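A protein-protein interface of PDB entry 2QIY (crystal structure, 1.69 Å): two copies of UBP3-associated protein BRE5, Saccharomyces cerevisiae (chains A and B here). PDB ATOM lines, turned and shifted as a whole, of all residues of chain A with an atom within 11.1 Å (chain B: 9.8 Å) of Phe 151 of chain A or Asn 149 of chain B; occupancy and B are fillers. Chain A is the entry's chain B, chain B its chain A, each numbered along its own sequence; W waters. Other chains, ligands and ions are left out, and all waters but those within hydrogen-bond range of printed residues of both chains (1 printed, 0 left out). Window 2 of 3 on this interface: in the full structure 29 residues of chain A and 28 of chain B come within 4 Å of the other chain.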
ATOM      1  N   ASP A  58      -1.120  -6.183  27.970  1.00  0.00           N
ATOM      2  CA  ASP A  58      -0.524  -5.023  27.338  1.00  0.00           C
ATOM      3  C   ASP A  58      -1.590  -3.964  27.100  1.00  0.00           C
ATOM      4  O   ASP A  58      -1.362  -3.011  26.367  1.00  0.00           O
ATOM      5  CB  ASP A  58       0.201  -5.401  26.033  1.00  0.00           C
ATOM      6  CG  ASP A  58      -0.707  -6.073  25.006  1.00  0.00           C
ATOM      7  OD1 ASP A  58      -0.196  -6.432  23.927  1.00  0.00           O
ATOM      8  OD2 ASP A  58      -1.922  -6.244  25.256  1.00  0.00           O
ATOM      9  N   VAL A  59      -2.751  -4.158  27.725  1.00  0.00           N
ATOM     10  CA  VAL A  59      -3.802  -3.137  27.773  1.00  0.00           C
ATOM     11  C   VAL A  59      -4.280  -2.895  29.215  1.00  0.00           C
ATOM     12  O   VAL A  59      -4.062  -3.729  30.096  1.00  0.00           O
ATOM     13  CB  VAL A  59      -5.030  -3.483  26.879  1.00  0.00           C
ATOM     14  CG1 VAL A  59      -4.633  -3.610  25.414  1.00  0.00           C
ATOM     15  CG2 VAL A  59      -5.758  -4.717  27.360  1.00  0.00           C
ATOM     16  N   LYS A  88       5.764   8.323  24.673  1.00  0.00           N
ATOM     17  CA  LYS A  88       6.328   8.632  23.378  1.00  0.00           C
ATOM     18  C   LYS A  88       5.141   8.904  22.462  1.00  0.00           C
ATOM     19  O   LYS A  88       4.302   8.028  22.251  1.00  0.00           O
ATOM     20  CB  LYS A  88       7.108   7.447  22.850  1.00  0.00           C
ATOM     21  CG  LYS A  88       7.648   7.630  21.440  1.00  0.00           C
ATOM     22  CD  LYS A  88       8.389   6.375  21.032  1.00  0.00           C
ATOM     23  CE  LYS A  88       9.063   6.533  19.693  1.00  0.00           C
ATOM     24  NZ  LYS A  88       9.580   5.217  19.216  1.00  0.00           N
ATOM     25  N   ASP A  90       3.743   9.409  18.936  1.00  0.00           N
ATOM     26  CA  ASP A  90       4.181   9.021  17.591  1.00  0.00           C
ATOM     27  C   ASP A  90       3.482   9.815  16.484  1.00  0.00           C
ATOM     28  O   ASP A  90       4.094  10.166  15.468  1.00  0.00           O
ATOM     29  CB  ASP A  90       3.845   7.553  17.327  1.00  0.00           C
ATOM     30  CG  ASP A  90       4.768   6.571  18.052  1.00  0.00           C
ATOM     31  OD1 ASP A  90       4.260   5.482  18.426  1.00  0.00           O
ATOM     32  OD2 ASP A  90       5.988   6.855  18.225  1.00  0.00           O
ATOM     33  N   THR A  91       2.184  10.042  16.667  1.00  0.00           N
ATOM     34  CA  THR A  91       1.367  10.610  15.586  1.00  0.00           C
ATOM     35  C   THR A  91       0.292  11.554  16.119  1.00  0.00           C
ATOM     36  O   THR A  91      -0.220  11.393  17.246  1.00  0.00           O
ATOM     37  CB  THR A  91       0.652   9.518  14.728  1.00  0.00           C
ATOM     38  OG1 THR A  91      -0.414   8.921  15.492  1.00  0.00           O
ATOM     39  CG2 THR A  91       1.619   8.416  14.233  1.00  0.00           C
ATOM     40  N   THR A 109      -1.514   9.066  18.796  1.00  0.00           N
ATOM     41  CA  THR A 109      -1.123   7.680  19.105  1.00  0.00           C
ATOM     42  C   THR A 109       0.293   7.641  19.598  1.00  0.00           C
ATOM     43  O   THR A 109       1.106   8.513  19.277  1.00  0.00           O
ATOM     44  CB  THR A 109      -1.294   6.678  17.942  1.00  0.00           C
ATOM     45  OG1 THR A 109      -0.199   6.795  17.010  1.00  0.00           O
ATOM     46  CG2 THR A 109      -2.663   6.871  17.270  1.00  0.00           C
ATOM     47  N   GLY A 110       0.593   6.617  20.378  1.00  0.00           N
ATOM     48  CA  GLY A 110       1.943   6.445  20.865  1.00  0.00           C
ATOM     49  C   GLY A 110       2.065   5.288  21.811  1.00  0.00           C
ATOM     50  O   GLY A 110       1.280   4.335  21.752  1.00  0.00           O
ATOM     51  N   GLU A 111       3.050   5.400  22.695  1.00  0.00           N
ATOM     52  CA  GLU A 111       3.288   4.385  23.706  1.00  0.00           C
ATOM     53  C   GLU A 111       3.394   5.093  25.038  1.00  0.00           C
ATOM     54  O   GLU A 111       4.187   6.029  25.187  1.00  0.00           O
ATOM     55  CB  GLU A 111       4.561   3.594  23.391  1.00  0.00           C
ATOM     56  CG  GLU A 111       4.419   2.743  22.119  1.00  0.00           C
ATOM     57  CD  GLU A 111       5.647   1.941  21.804  1.00  0.00           C
ATOM     58  OE1 GLU A 111       6.054   1.141  22.653  1.00  0.00           O
ATOM     59  OE2 GLU A 111       6.192   2.096  20.698  1.00  0.00           O
ATOM     60  N   VAL A 119       5.654  -0.411  28.605  1.00  0.00           N
ATOM     61  CA  VAL A 119       4.897   0.481  27.732  1.00  0.00           C
ATOM     62  C   VAL A 119       3.572  -0.155  27.340  1.00  0.00           C
ATOM     63  O   VAL A 119       3.454  -1.404  27.325  1.00  0.00           O
ATOM     64  CB  VAL A 119       5.681   0.834  26.420  1.00  0.00           C
ATOM     65  CG1 VAL A 119       6.939   1.625  26.746  1.00  0.00           C
ATOM     66  CG2 VAL A 119       6.025  -0.431  25.640  1.00  0.00           C
ATOM     67  N   TYR A 120       2.598   0.713  27.030  1.00  0.00           N
ATOM     68  CA  TYR A 120       1.302   0.330  26.508  1.00  0.00           C
ATOM     69  C   TYR A 120       1.075   1.177  25.262  1.00  0.00           C
ATOM     70  O   TYR A 120       1.204   2.408  25.301  1.00  0.00           O
ATOM     71  CB  TYR A 120       0.190   0.616  27.529  1.00  0.00           C
ATOM     72  CG  TYR A 120       0.330  -0.157  28.813  1.00  0.00           C
ATOM     73  CD1 TYR A 120       1.168   0.293  29.814  1.00  0.00           C
ATOM     74  CD2 TYR A 120      -0.398  -1.322  29.030  1.00  0.00           C
ATOM     75  CE1 TYR A 120       1.314  -0.405  30.996  1.00  0.00           C
ATOM     76  CE2 TYR A 120      -0.265  -2.040  30.219  1.00  0.00           C
ATOM     77  CZ  TYR A 120       0.596  -1.570  31.197  1.00  0.00           C
ATOM     78  OH  TYR A 120       0.749  -2.239  32.383  1.00  0.00           O
ATOM     79  N   LYS A 121       0.714   0.526  24.172  1.00  0.00           N
ATOM     80  CA  LYS A 121       0.359   1.228  22.947  1.00  0.00           C
ATOM     81  C   LYS A 121      -1.011   1.877  23.167  1.00  0.00           C
ATOM     82  O   LYS A 121      -1.915   1.262  23.717  1.00  0.00           O
ATOM     83  CB  LYS A 121       0.306   0.229  21.785  1.00  0.00           C
ATOM     84  CG  LYS A 121       0.032   0.868  20.428  1.00  0.00           C
ATOM     85  CD  LYS A 121       1.281   1.477  19.797  1.00  0.00           C
ATOM     86  CE  LYS A 121       2.140   0.383  19.135  1.00  0.00           C
ATOM     87  NZ  LYS A 121       3.255   0.948  18.329  1.00  0.00           N
ATOM     88  N   PHE A 122      -1.172   3.120  22.718  1.00  0.00           N
ATOM     89  CA  PHE A 122      -2.463   3.780  22.894  1.00  0.00           C
ATOM     90  C   PHE A 122      -2.866   4.651  21.740  1.00  0.00           C
ATOM     91  O   PHE A 122      -2.028   5.097  20.943  1.00  0.00           O
ATOM     92  CB  PHE A 122      -2.463   4.656  24.166  1.00  0.00           C
ATOM     93  CG  PHE A 122      -1.738   5.952  23.990  1.00  0.00           C
ATOM     94  CD1 PHE A 122      -2.449   7.126  23.681  1.00  0.00           C
ATOM     95  CD2 PHE A 122      -0.343   6.000  24.078  1.00  0.00           C
ATOM     96  CE1 PHE A 122      -1.774   8.341  23.482  1.00  0.00           C
ATOM     97  CE2 PHE A 122       0.342   7.194  23.889  1.00  0.00           C
ATOM     98  CZ  PHE A 122      -0.372   8.370  23.578  1.00  0.00           C
ATOM     99  N   PHE A 146      -6.277   1.595  24.913  1.00  0.00           N
ATOM    100  CA  PHE A 146      -5.038   0.859  24.754  1.00  0.00           C
ATOM    101  C   PHE A 146      -5.183  -0.238  23.703  1.00  0.00           C
ATOM    102  O   PHE A 146      -6.257  -0.838  23.551  1.00  0.00           O
ATOM    103  CB  PHE A 146      -4.538   0.320  26.106  1.00  0.00           C
ATOM    104  CG  PHE A 146      -4.266   1.432  27.093  1.00  0.00           C
ATOM    105  CD1 PHE A 146      -3.074   2.160  27.004  1.00  0.00           C
ATOM    106  CD2 PHE A 146      -5.245   1.835  27.994  1.00  0.00           C
ATOM    107  CE1 PHE A 146      -2.812   3.218  27.848  1.00  0.00           C
ATOM    108  CE2 PHE A 146      -4.997   2.904  28.868  1.00  0.00           C
ATOM    109  CZ  PHE A 146      -3.767   3.598  28.782  1.00  0.00           C
ATOM    110  N   ILE A 147      -4.089  -0.473  22.983  1.00  0.00           N
ATOM    111  CA  ILE A 147      -4.064  -1.338  21.809  1.00  0.00           C
ATOM    112  C   ILE A 147      -3.148  -2.519  22.074  1.00  0.00           C
ATOM    113  O   ILE A 147      -1.958  -2.353  22.307  1.00  0.00           O
ATOM    114  CB  ILE A 147      -3.499  -0.580  20.580  1.00  0.00           C
ATOM    115  CG1 ILE A 147      -4.157   0.802  20.421  1.00  0.00           C
ATOM    116  CG2 ILE A 147      -3.542  -1.463  19.317  1.00  0.00           C
ATOM    117  CD1 ILE A 147      -5.421   0.841  19.630  1.00  0.00           C
ATOM    118  N   SER A 148      -3.708  -3.711  21.980  1.00  0.00           N
ATOM    119  CA  SER A 148      -2.953  -4.918  22.265  1.00  0.00           C
ATOM    120  C   SER A 148      -2.189  -5.338  21.012  1.00  0.00           C
ATOM    121  O   SER A 148      -2.585  -4.997  19.905  1.00  0.00           O
ATOM    122  CB  SER A 148      -3.916  -6.010  22.684  1.00  0.00           C
ATOM    123  OG  SER A 148      -4.956  -6.102  21.725  1.00  0.00           O
ATOM    124  N   ASN A 149      -1.089  -6.063  21.188  1.00  0.00           N
ATOM    125  CA  ASN A 149      -0.265  -6.463  20.048  1.00  0.00           C
ATOM    126  C   ASN A 149      -0.965  -7.447  19.125  1.00  0.00           C
ATOM    127  O   ASN A 149      -1.775  -8.261  19.578  1.00  0.00           O
ATOM    128  CB  ASN A 149       1.064  -7.068  20.501  1.00  0.00           C
ATOM    129  CG  ASN A 149       2.201  -6.065  20.448  1.00  0.00           C
ATOM    130  OD1 ASN A 149       2.334  -5.207  21.331  1.00  0.00           O
ATOM    131  ND2 ASN A 149       3.034  -6.170  19.416  1.00  0.00           N
ATOM    132  N   SER A 150      -0.630  -7.376  17.840  1.00  0.00           N
ATOM    133  CA  SER A 150      -1.226  -8.251  16.817  1.00  0.00           C
ATOM    134  C   SER A 150      -0.857  -9.701  17.070  1.00  0.00           C
ATOM    135  O   SER A 150      -1.568 -10.618  16.630  1.00  0.00           O
ATOM    136  CB  SER A 150      -0.756  -7.831  15.428  1.00  0.00           C
ATOM    137  OG  SER A 150      -1.029  -6.456  15.200  1.00  0.00           O
ATOM    138  N   PHE A 151       0.248  -9.899  17.795  1.00  0.00           N
ATOM    139  CA  PHE A 151       0.869 -11.212  17.954  1.00  0.00           C
ATOM    140  C   PHE A 151       1.062 -11.563  19.427  1.00  0.00           C
ATOM    141  O   PHE A 151       1.063 -12.735  19.814  1.00  0.00           O
ATOM    142  CB  PHE A 151       2.200 -11.258  17.197  1.00  0.00           C
ATOM    143  CG  PHE A 151       2.068 -10.937  15.719  1.00  0.00           C
ATOM    144  CD1 PHE A 151       1.066 -11.537  14.946  1.00  0.00           C
ATOM    145  CD2 PHE A 151       2.950 -10.064  15.100  1.00  0.00           C
ATOM    146  CE1 PHE A 151       0.913 -11.239  13.591  1.00  0.00           C
ATOM    147  CE2 PHE A 151       2.814  -9.764  13.738  1.00  0.00           C
ATOM    148  CZ  PHE A 151       1.790 -10.360  12.985  1.00  0.00           C
ATOM    149  N   LYS B  56       7.923  -5.164   4.868  1.00  0.00           N
ATOM    150  CA  LYS B  56       7.436  -3.954   4.261  1.00  0.00           C
ATOM    151  C   LYS B  56       6.606  -3.169   5.292  1.00  0.00           C
ATOM    152  O   LYS B  56       6.516  -3.535   6.481  1.00  0.00           O
ATOM    153  CB  LYS B  56       6.634  -4.246   2.979  1.00  0.00           C
ATOM    154  CG  LYS B  56       5.290  -4.921   3.215  1.00  0.00           C
ATOM    155  CD  LYS B  56       4.279  -4.558   2.140  1.00  0.00           C
ATOM    156  CE  LYS B  56       2.877  -5.037   2.532  1.00  0.00           C
ATOM    157  NZ  LYS B  56       2.106  -5.578   1.355  1.00  0.00           N
ATOM    158  N   ASP B  57       6.014  -2.082   4.819  1.00  0.00           N
ATOM    159  CA  ASP B  57       5.341  -1.115   5.673  1.00  0.00           C
ATOM    160  C   ASP B  57       4.147  -1.720   6.368  1.00  0.00           C
ATOM    161  O   ASP B  57       3.308  -2.344   5.732  1.00  0.00           O
ATOM    162  CB  ASP B  57       4.839   0.069   4.843  1.00  0.00           C
ATOM    163  CG  ASP B  57       5.951   0.801   4.099  1.00  0.00           C
ATOM    164  OD1 ASP B  57       5.607   1.619   3.203  1.00  0.00           O
ATOM    165  OD2 ASP B  57       7.149   0.586   4.407  1.00  0.00           O
ATOM    166  N   ASP B  58       4.049  -1.516   7.674  1.00  0.00           N
ATOM    167  CA  ASP B  58       2.858  -1.977   8.350  1.00  0.00           C
ATOM    168  C   ASP B  58       1.954  -0.811   8.711  1.00  0.00           C
ATOM    169  O   ASP B  58       1.014  -0.958   9.483  1.00  0.00           O
ATOM    170  CB  ASP B  58       3.204  -2.871   9.536  1.00  0.00           C
ATOM    171  CG  ASP B  58       3.784  -2.107  10.718  1.00  0.00           C
ATOM    172  OD1 ASP B  58       3.802  -2.713  11.810  1.00  0.00           O
ATOM    173  OD2 ASP B  58       4.187  -0.924  10.568  1.00  0.00           O
ATOM    174  N   VAL B  59       2.238   0.355   8.123  1.00  0.00           N
ATOM    175  CA  VAL B  59       1.270   1.447   8.132  1.00  0.00           C
ATOM    176  C   VAL B  59       1.020   1.949   6.707  1.00  0.00           C
ATOM    177  O   VAL B  59       1.806   1.684   5.784  1.00  0.00           O
ATOM    178  CB  VAL B  59       1.704   2.637   9.023  1.00  0.00           C
ATOM    179  CG1 VAL B  59       1.857   2.207  10.486  1.00  0.00           C
ATOM    180  CG2 VAL B  59       3.000   3.292   8.480  1.00  0.00           C
ATOM    181  N   LEU B  60      -0.081   2.665   6.533  1.00  0.00           N
ATOM    182  CA  LEU B  60      -0.386   3.251   5.236  1.00  0.00           C
ATOM    183  C   LEU B  60      -0.563   4.736   5.430  1.00  0.00           C
ATOM    184  O   LEU B  60      -0.988   5.170   6.516  1.00  0.00           O
ATOM    185  CB  LEU B  60      -1.682   2.675   4.664  1.00  0.00           C
ATOM    186  CG  LEU B  60      -1.643   1.165   4.397  1.00  0.00           C
ATOM    187  CD1 LEU B  60      -3.039   0.695   4.142  1.00  0.00           C
ATOM    188  CD2 LEU B  60      -0.740   0.809   3.236  1.00  0.00           C
ATOM    189  N   LYS B  88     -11.112  -6.802  11.180  1.00  0.00           N
ATOM    190  CA  LYS B  88     -11.456  -7.313  12.497  1.00  0.00           C
ATOM    191  C   LYS B  88     -11.652  -6.089  13.379  1.00  0.00           C
ATOM    192  O   LYS B  88     -10.720  -5.298  13.572  1.00  0.00           O
ATOM    193  CB  LYS B  88     -10.332  -8.192  13.026  1.00  0.00           C
ATOM    194  CG  LYS B  88     -10.572  -8.682  14.439  1.00  0.00           C
ATOM    195  CD  LYS B  88      -9.486  -9.647  14.900  1.00  0.00           C
ATOM    196  CE  LYS B  88      -9.785 -10.111  16.314  1.00  0.00           C
ATOM    197  NZ  LYS B  88      -8.817 -11.147  16.767  1.00  0.00           N
ATOM    198  N   ASP B  90     -12.028  -4.579  16.858  1.00  0.00           N
ATOM    199  CA  ASP B  90     -11.661  -5.031  18.213  1.00  0.00           C
ATOM    200  C   ASP B  90     -12.379  -4.276  19.345  1.00  0.00           C
ATOM    201  O   ASP B  90     -12.782  -4.875  20.350  1.00  0.00           O
ATOM    202  CB  ASP B  90     -10.161  -4.860  18.461  1.00  0.00           C
ATOM    203  CG  ASP B  90      -9.296  -5.864  17.697  1.00  0.00           C
ATOM    204  OD1 ASP B  90      -8.207  -5.441  17.281  1.00  0.00           O
ATOM    205  OD2 ASP B  90      -9.661  -7.053  17.546  1.00  0.00           O
ATOM    206  N   GLY B 110      -8.887  -1.747  15.442  1.00  0.00           N
ATOM    207  CA  GLY B 110      -8.928  -3.118  14.930  1.00  0.00           C
ATOM    208  C   GLY B 110      -7.777  -3.365  13.991  1.00  0.00           C
ATOM    209  O   GLY B 110      -6.764  -2.654  14.040  1.00  0.00           O
ATOM    210  N   GLU B 111      -7.958  -4.353  13.125  1.00  0.00           N
ATOM    211  CA  GLU B 111      -6.955  -4.712  12.124  1.00  0.00           C
ATOM    212  C   GLU B 111      -7.663  -4.788  10.781  1.00  0.00           C
ATOM    213  O   GLU B 111      -8.664  -5.475  10.640  1.00  0.00           O
ATOM    214  CB  GLU B 111      -6.249  -6.012  12.507  1.00  0.00           C
ATOM    215  CG  GLU B 111      -5.441  -5.828  13.811  1.00  0.00           C
ATOM    216  CD  GLU B 111      -4.441  -6.930  14.131  1.00  0.00           C
ATOM    217  OE1 GLU B 111      -4.250  -7.873  13.335  1.00  0.00           O
ATOM    218  OE2 GLU B 111      -3.782  -6.772  15.195  1.00  0.00           O
ATOM    219  N   PRO B 118      -1.671  -8.120   3.632  1.00  0.00           N
ATOM    220  CA  PRO B 118      -1.512  -8.309   5.078  1.00  0.00           C
ATOM    221  C   PRO B 118      -2.404  -7.348   5.855  1.00  0.00           C
ATOM    222  O   PRO B 118      -2.966  -6.404   5.282  1.00  0.00           O
ATOM    223  CB  PRO B 118      -0.048  -7.956   5.342  1.00  0.00           C
ATOM    224  CG  PRO B 118       0.360  -7.137   4.176  1.00  0.00           C
ATOM    225  CD  PRO B 118      -0.464  -7.539   3.008  1.00  0.00           C
ATOM    226  N   VAL B 119      -2.495  -7.566   7.167  1.00  0.00           N
ATOM    227  CA  VAL B 119      -3.251  -6.649   8.026  1.00  0.00           C
ATOM    228  C   VAL B 119      -2.437  -5.385   8.377  1.00  0.00           C
ATOM    229  O   VAL B 119      -1.195  -5.365   8.308  1.00  0.00           O
ATOM    230  CB  VAL B 119      -3.664  -7.292   9.349  1.00  0.00           C
ATOM    231  CG1 VAL B 119      -4.625  -8.458   9.083  1.00  0.00           C
ATOM    232  CG2 VAL B 119      -2.406  -7.768  10.138  1.00  0.00           C
ATOM    233  N   TYR B 120      -3.193  -4.356   8.773  1.00  0.00           N
ATOM    234  CA  TYR B 120      -2.668  -3.104   9.281  1.00  0.00           C
ATOM    235  C   TYR B 120      -3.521  -2.722  10.483  1.00  0.00           C
ATOM    236  O   TYR B 120      -4.768  -2.720  10.391  1.00  0.00           O
ATOM    237  CB  TYR B 120      -2.847  -2.016   8.234  1.00  0.00           C
ATOM    238  CG  TYR B 120      -2.130  -2.281   6.940  1.00  0.00           C
ATOM    239  CD1 TYR B 120      -2.692  -3.093   5.963  1.00  0.00           C
ATOM    240  CD2 TYR B 120      -0.880  -1.715   6.702  1.00  0.00           C
ATOM    241  CE1 TYR B 120      -2.048  -3.332   4.748  1.00  0.00           C
ATOM    242  CE2 TYR B 120      -0.217  -1.928   5.511  1.00  0.00           C
ATOM    243  CZ  TYR B 120      -0.804  -2.757   4.524  1.00  0.00           C
ATOM    244  OH  TYR B 120      -0.143  -3.014   3.340  1.00  0.00           O
ATOM    245  N   LYS B 121      -2.879  -2.402  11.598  1.00  0.00           N
ATOM    246  CA  LYS B 121      -3.599  -2.010  12.818  1.00  0.00           C
ATOM    247  C   LYS B 121      -4.105  -0.615  12.592  1.00  0.00           C
ATOM    248  O   LYS B 121      -3.397   0.188  11.982  1.00  0.00           O
ATOM    249  CB  LYS B 121      -2.655  -1.940  13.997  1.00  0.00           C
ATOM    250  CG  LYS B 121      -2.344  -3.277  14.632  1.00  0.00           C
ATOM    251  CD  LYS B 121      -1.928  -2.982  16.088  1.00  0.00           C
ATOM    252  CE  LYS B 121      -2.201  -4.160  17.027  1.00  0.00           C
ATOM    253  NZ  LYS B 121      -3.599  -4.637  17.069  1.00  0.00           N
ATOM    254  N   PHE B 122      -5.310  -0.307  13.070  1.00  0.00           N
ATOM    255  CA  PHE B 122      -5.822   1.056  12.872  1.00  0.00           C
ATOM    256  C   PHE B 122      -6.659   1.506  14.046  1.00  0.00           C
ATOM    257  O   PHE B 122      -7.175   0.701  14.820  1.00  0.00           O
ATOM    258  CB  PHE B 122      -6.700   1.113  11.607  1.00  0.00           C
ATOM    259  CG  PHE B 122      -8.079   0.505  11.801  1.00  0.00           C
ATOM    260  CD1 PHE B 122      -9.146   1.328  12.183  1.00  0.00           C
ATOM    261  CD2 PHE B 122      -8.298  -0.863  11.662  1.00  0.00           C
ATOM    262  CE1 PHE B 122     -10.406   0.812  12.391  1.00  0.00           C
ATOM    263  CE2 PHE B 122      -9.555  -1.393  11.857  1.00  0.00           C
ATOM    264  CZ  PHE B 122     -10.626  -0.557  12.227  1.00  0.00           C
ATOM    265  N   PHE B 146      -3.272   4.597  10.858  1.00  0.00           N
ATOM    266  CA  PHE B 146      -2.629   3.289  10.973  1.00  0.00           C
ATOM    267  C   PHE B 146      -1.495   3.327  11.979  1.00  0.00           C
ATOM    268  O   PHE B 146      -0.752   4.303  12.071  1.00  0.00           O
ATOM    269  CB  PHE B 146      -2.190   2.787   9.583  1.00  0.00           C
ATOM    270  CG  PHE B 146      -3.349   2.582   8.679  1.00  0.00           C
ATOM    271  CD1 PHE B 146      -4.104   1.399   8.757  1.00  0.00           C
ATOM    272  CD2 PHE B 146      -3.750   3.575   7.789  1.00  0.00           C
ATOM    273  CE1 PHE B 146      -5.221   1.229   7.939  1.00  0.00           C
ATOM    274  CE2 PHE B 146      -4.872   3.418   6.965  1.00  0.00           C
ATOM    275  CZ  PHE B 146      -5.618   2.227   7.035  1.00  0.00           C
ATOM    276  N   ILE B 147      -1.406   2.259  12.756  1.00  0.00           N
ATOM    277  CA  ILE B 147      -0.536   2.171  13.918  1.00  0.00           C
ATOM    278  C   ILE B 147       0.467   1.056  13.638  1.00  0.00           C
ATOM    279  O   ILE B 147       0.083  -0.036  13.260  1.00  0.00           O
ATOM    280  CB  ILE B 147      -1.395   1.884  15.200  1.00  0.00           C
ATOM    281  CG1 ILE B 147      -2.476   2.989  15.364  1.00  0.00           C
ATOM    282  CG2 ILE B 147      -0.513   1.793  16.454  1.00  0.00           C
ATOM    283  CD1 ILE B 147      -3.376   2.863  16.604  1.00  0.00           C
ATOM    284  N   SER B 148       1.745   1.337  13.801  1.00  0.00           N
ATOM    285  CA  SER B 148       2.723   0.273  13.632  1.00  0.00           C
ATOM    286  C   SER B 148       2.594  -0.680  14.823  1.00  0.00           C
ATOM    287  O   SER B 148       2.391  -0.239  15.963  1.00  0.00           O
ATOM    288  CB  SER B 148       4.127   0.854  13.535  1.00  0.00           C
ATOM    289  OG  SER B 148       4.943   0.056  12.691  1.00  0.00           O
ATOM    290  N   ASN B 149       2.687  -1.978  14.569  1.00  0.00           N
ATOM    291  CA  ASN B 149       2.657  -2.938  15.671  1.00  0.00           C
ATOM    292  C   ASN B 149       3.999  -2.987  16.391  1.00  0.00           C
ATOM    293  O   ASN B 149       4.946  -3.556  15.841  1.00  0.00           O
ATOM    294  CB  ASN B 149       2.306  -4.332  15.141  1.00  0.00           C
ATOM    295  CG  ASN B 149       1.943  -5.291  16.229  1.00  0.00           C
ATOM    296  OD1 ASN B 149       1.047  -5.034  17.043  1.00  0.00           O
ATOM    297  ND2 ASN B 149       2.620  -6.430  16.244  1.00  0.00           N
HETATM  298  O   HOH W   1      -3.058 -10.137  13.864  1.00  0.00           O
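Asn 149 of chain A touches just one residue of chain B: Asn 149. Ser 150 of chain A touches three residues of chain B. No residue of chain A comes within 4 Å of Asp 58 of chain B. Ser 148 of chain B touches just one residue of chain A: Lys 121. Printed residues of chain A within 4 Å of Glu 111 of chain B: Ser 150 (2.8 Å). Of the printed residues of chain B, Lys 121 of chain A touches Ile 147 (3.8 Å) and Ser 148 (2.8 Å). Printed residues of chain A within 4 Å of Ile 147 of chain B: Lys 121. Printed residues of chain B within 4 Å of Ser 148 of chain A: Lys 121. Printed residues of chain A within 4 Å of Lys 121 of chain B: Ile 147, Ser 148 and Ser 150. Tyr 120 of chain B touches none of the printed residues of chain A. The nearest residue of chain B that does not touch Phe 151 of chain A is Val 119 of chain B (5.7 Å).
OD2 of Asp 58 of chain B is in hydrogen-bond range of OG of Ser 148 of chain B (2.5 Å). N of Ile 147 of chain A sits at hydrogen-bond distance from O of Lys 121 of chain A, 2.9 Å away. N of Asn 149 of chain A lies within hydrogen-bond range of OD1 of Asp 58 of chain A. The backbone carbonyl oxygen (O) of Lys 121 of chain B sits at hydrogen-bond distance from the backbone NH (N) of Ile 147 of chain B. NZ of Lys 121 of chain A is in salt-bridge range of OE2 of Glu 111 of chain A (3.9 Å). N of Lys 88 of chain B is in hydrogen-bond range of O of Glu 111 of chain B, 2.8 Å away.
Lys 121 of chain A touches Ile 147 of chain B, and with the chains exchanged Ile 147 of chain A touches Lys 121 of chain B. Lys 121 of chain A touches Ser 148 of chain B, and with the chains exchanged Ser 148 of chain A touches Lys 121 of chain B. Asn 149 of chain B touches its own counterpart, Asn 149 of chain A. Of the 9 pairs that touch across the chains among the printed residues, 5 have their exchanged pair printed and touching as well.
Lys 121 of chain A touches Ile 147 of chain B. Lys 121 of chain B touches Ile 147 of chain A (CE to CG2, 3.8 Å). Ser 150 of chain A touches Lys 121 of chain B (OG to CE, 3.2 Å). ND2 of Asn 149 of chain B touches CD2 of Phe 151 of chain A, 3.8 Å away.
Printed residues of chain A that touch a printed residue of chain B: Lys 121, Ile 147, Ser 148, Asn 149, Ser 150 and Phe 151. Hydrophobic or aromatic side chains of chain A within 4 Å of the printed part of chain B: Ile 147 and Phe 151. Of the 18 printed residues of chain B, 5 touch a printed residue of chain A. Among the printed residues, no Asp or Glu carboxylate lies within 4 Å of a Lys or Arg side-chain nitrogen of the other chain.
Water W1 lies within hydrogen-bond range of the side-chain carboxylate (OE1) of Glu 111 of chain B and the backbone carbonyl oxygen (O) of Ser 150 of chain A.
The backbone carbonyl oxygen (O) of Ser 148 of chain B sits at hydrogen-bond distance from the side-chain amino group (NZ) of Lys 121 of chain A (2.8 Å). ND2 of Asn 149 of chain A sits close to ND2 of Asn 149 of chain B, at 3.2 Å. OE2 of Glu 111 of chain B is in hydrogen-bond range of OG of Ser 150 of chain A (2.8 Å). O of Ser 148 of chain A lies close to NZ of Lys 121 of chain B, at 3.0 Å. The side-chain amide oxygen (OD1) of Asn 149 of chain B lies within hydrogen-bond range of the backbone NH (N) of Ser 150 of chain A (3.0 Å).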
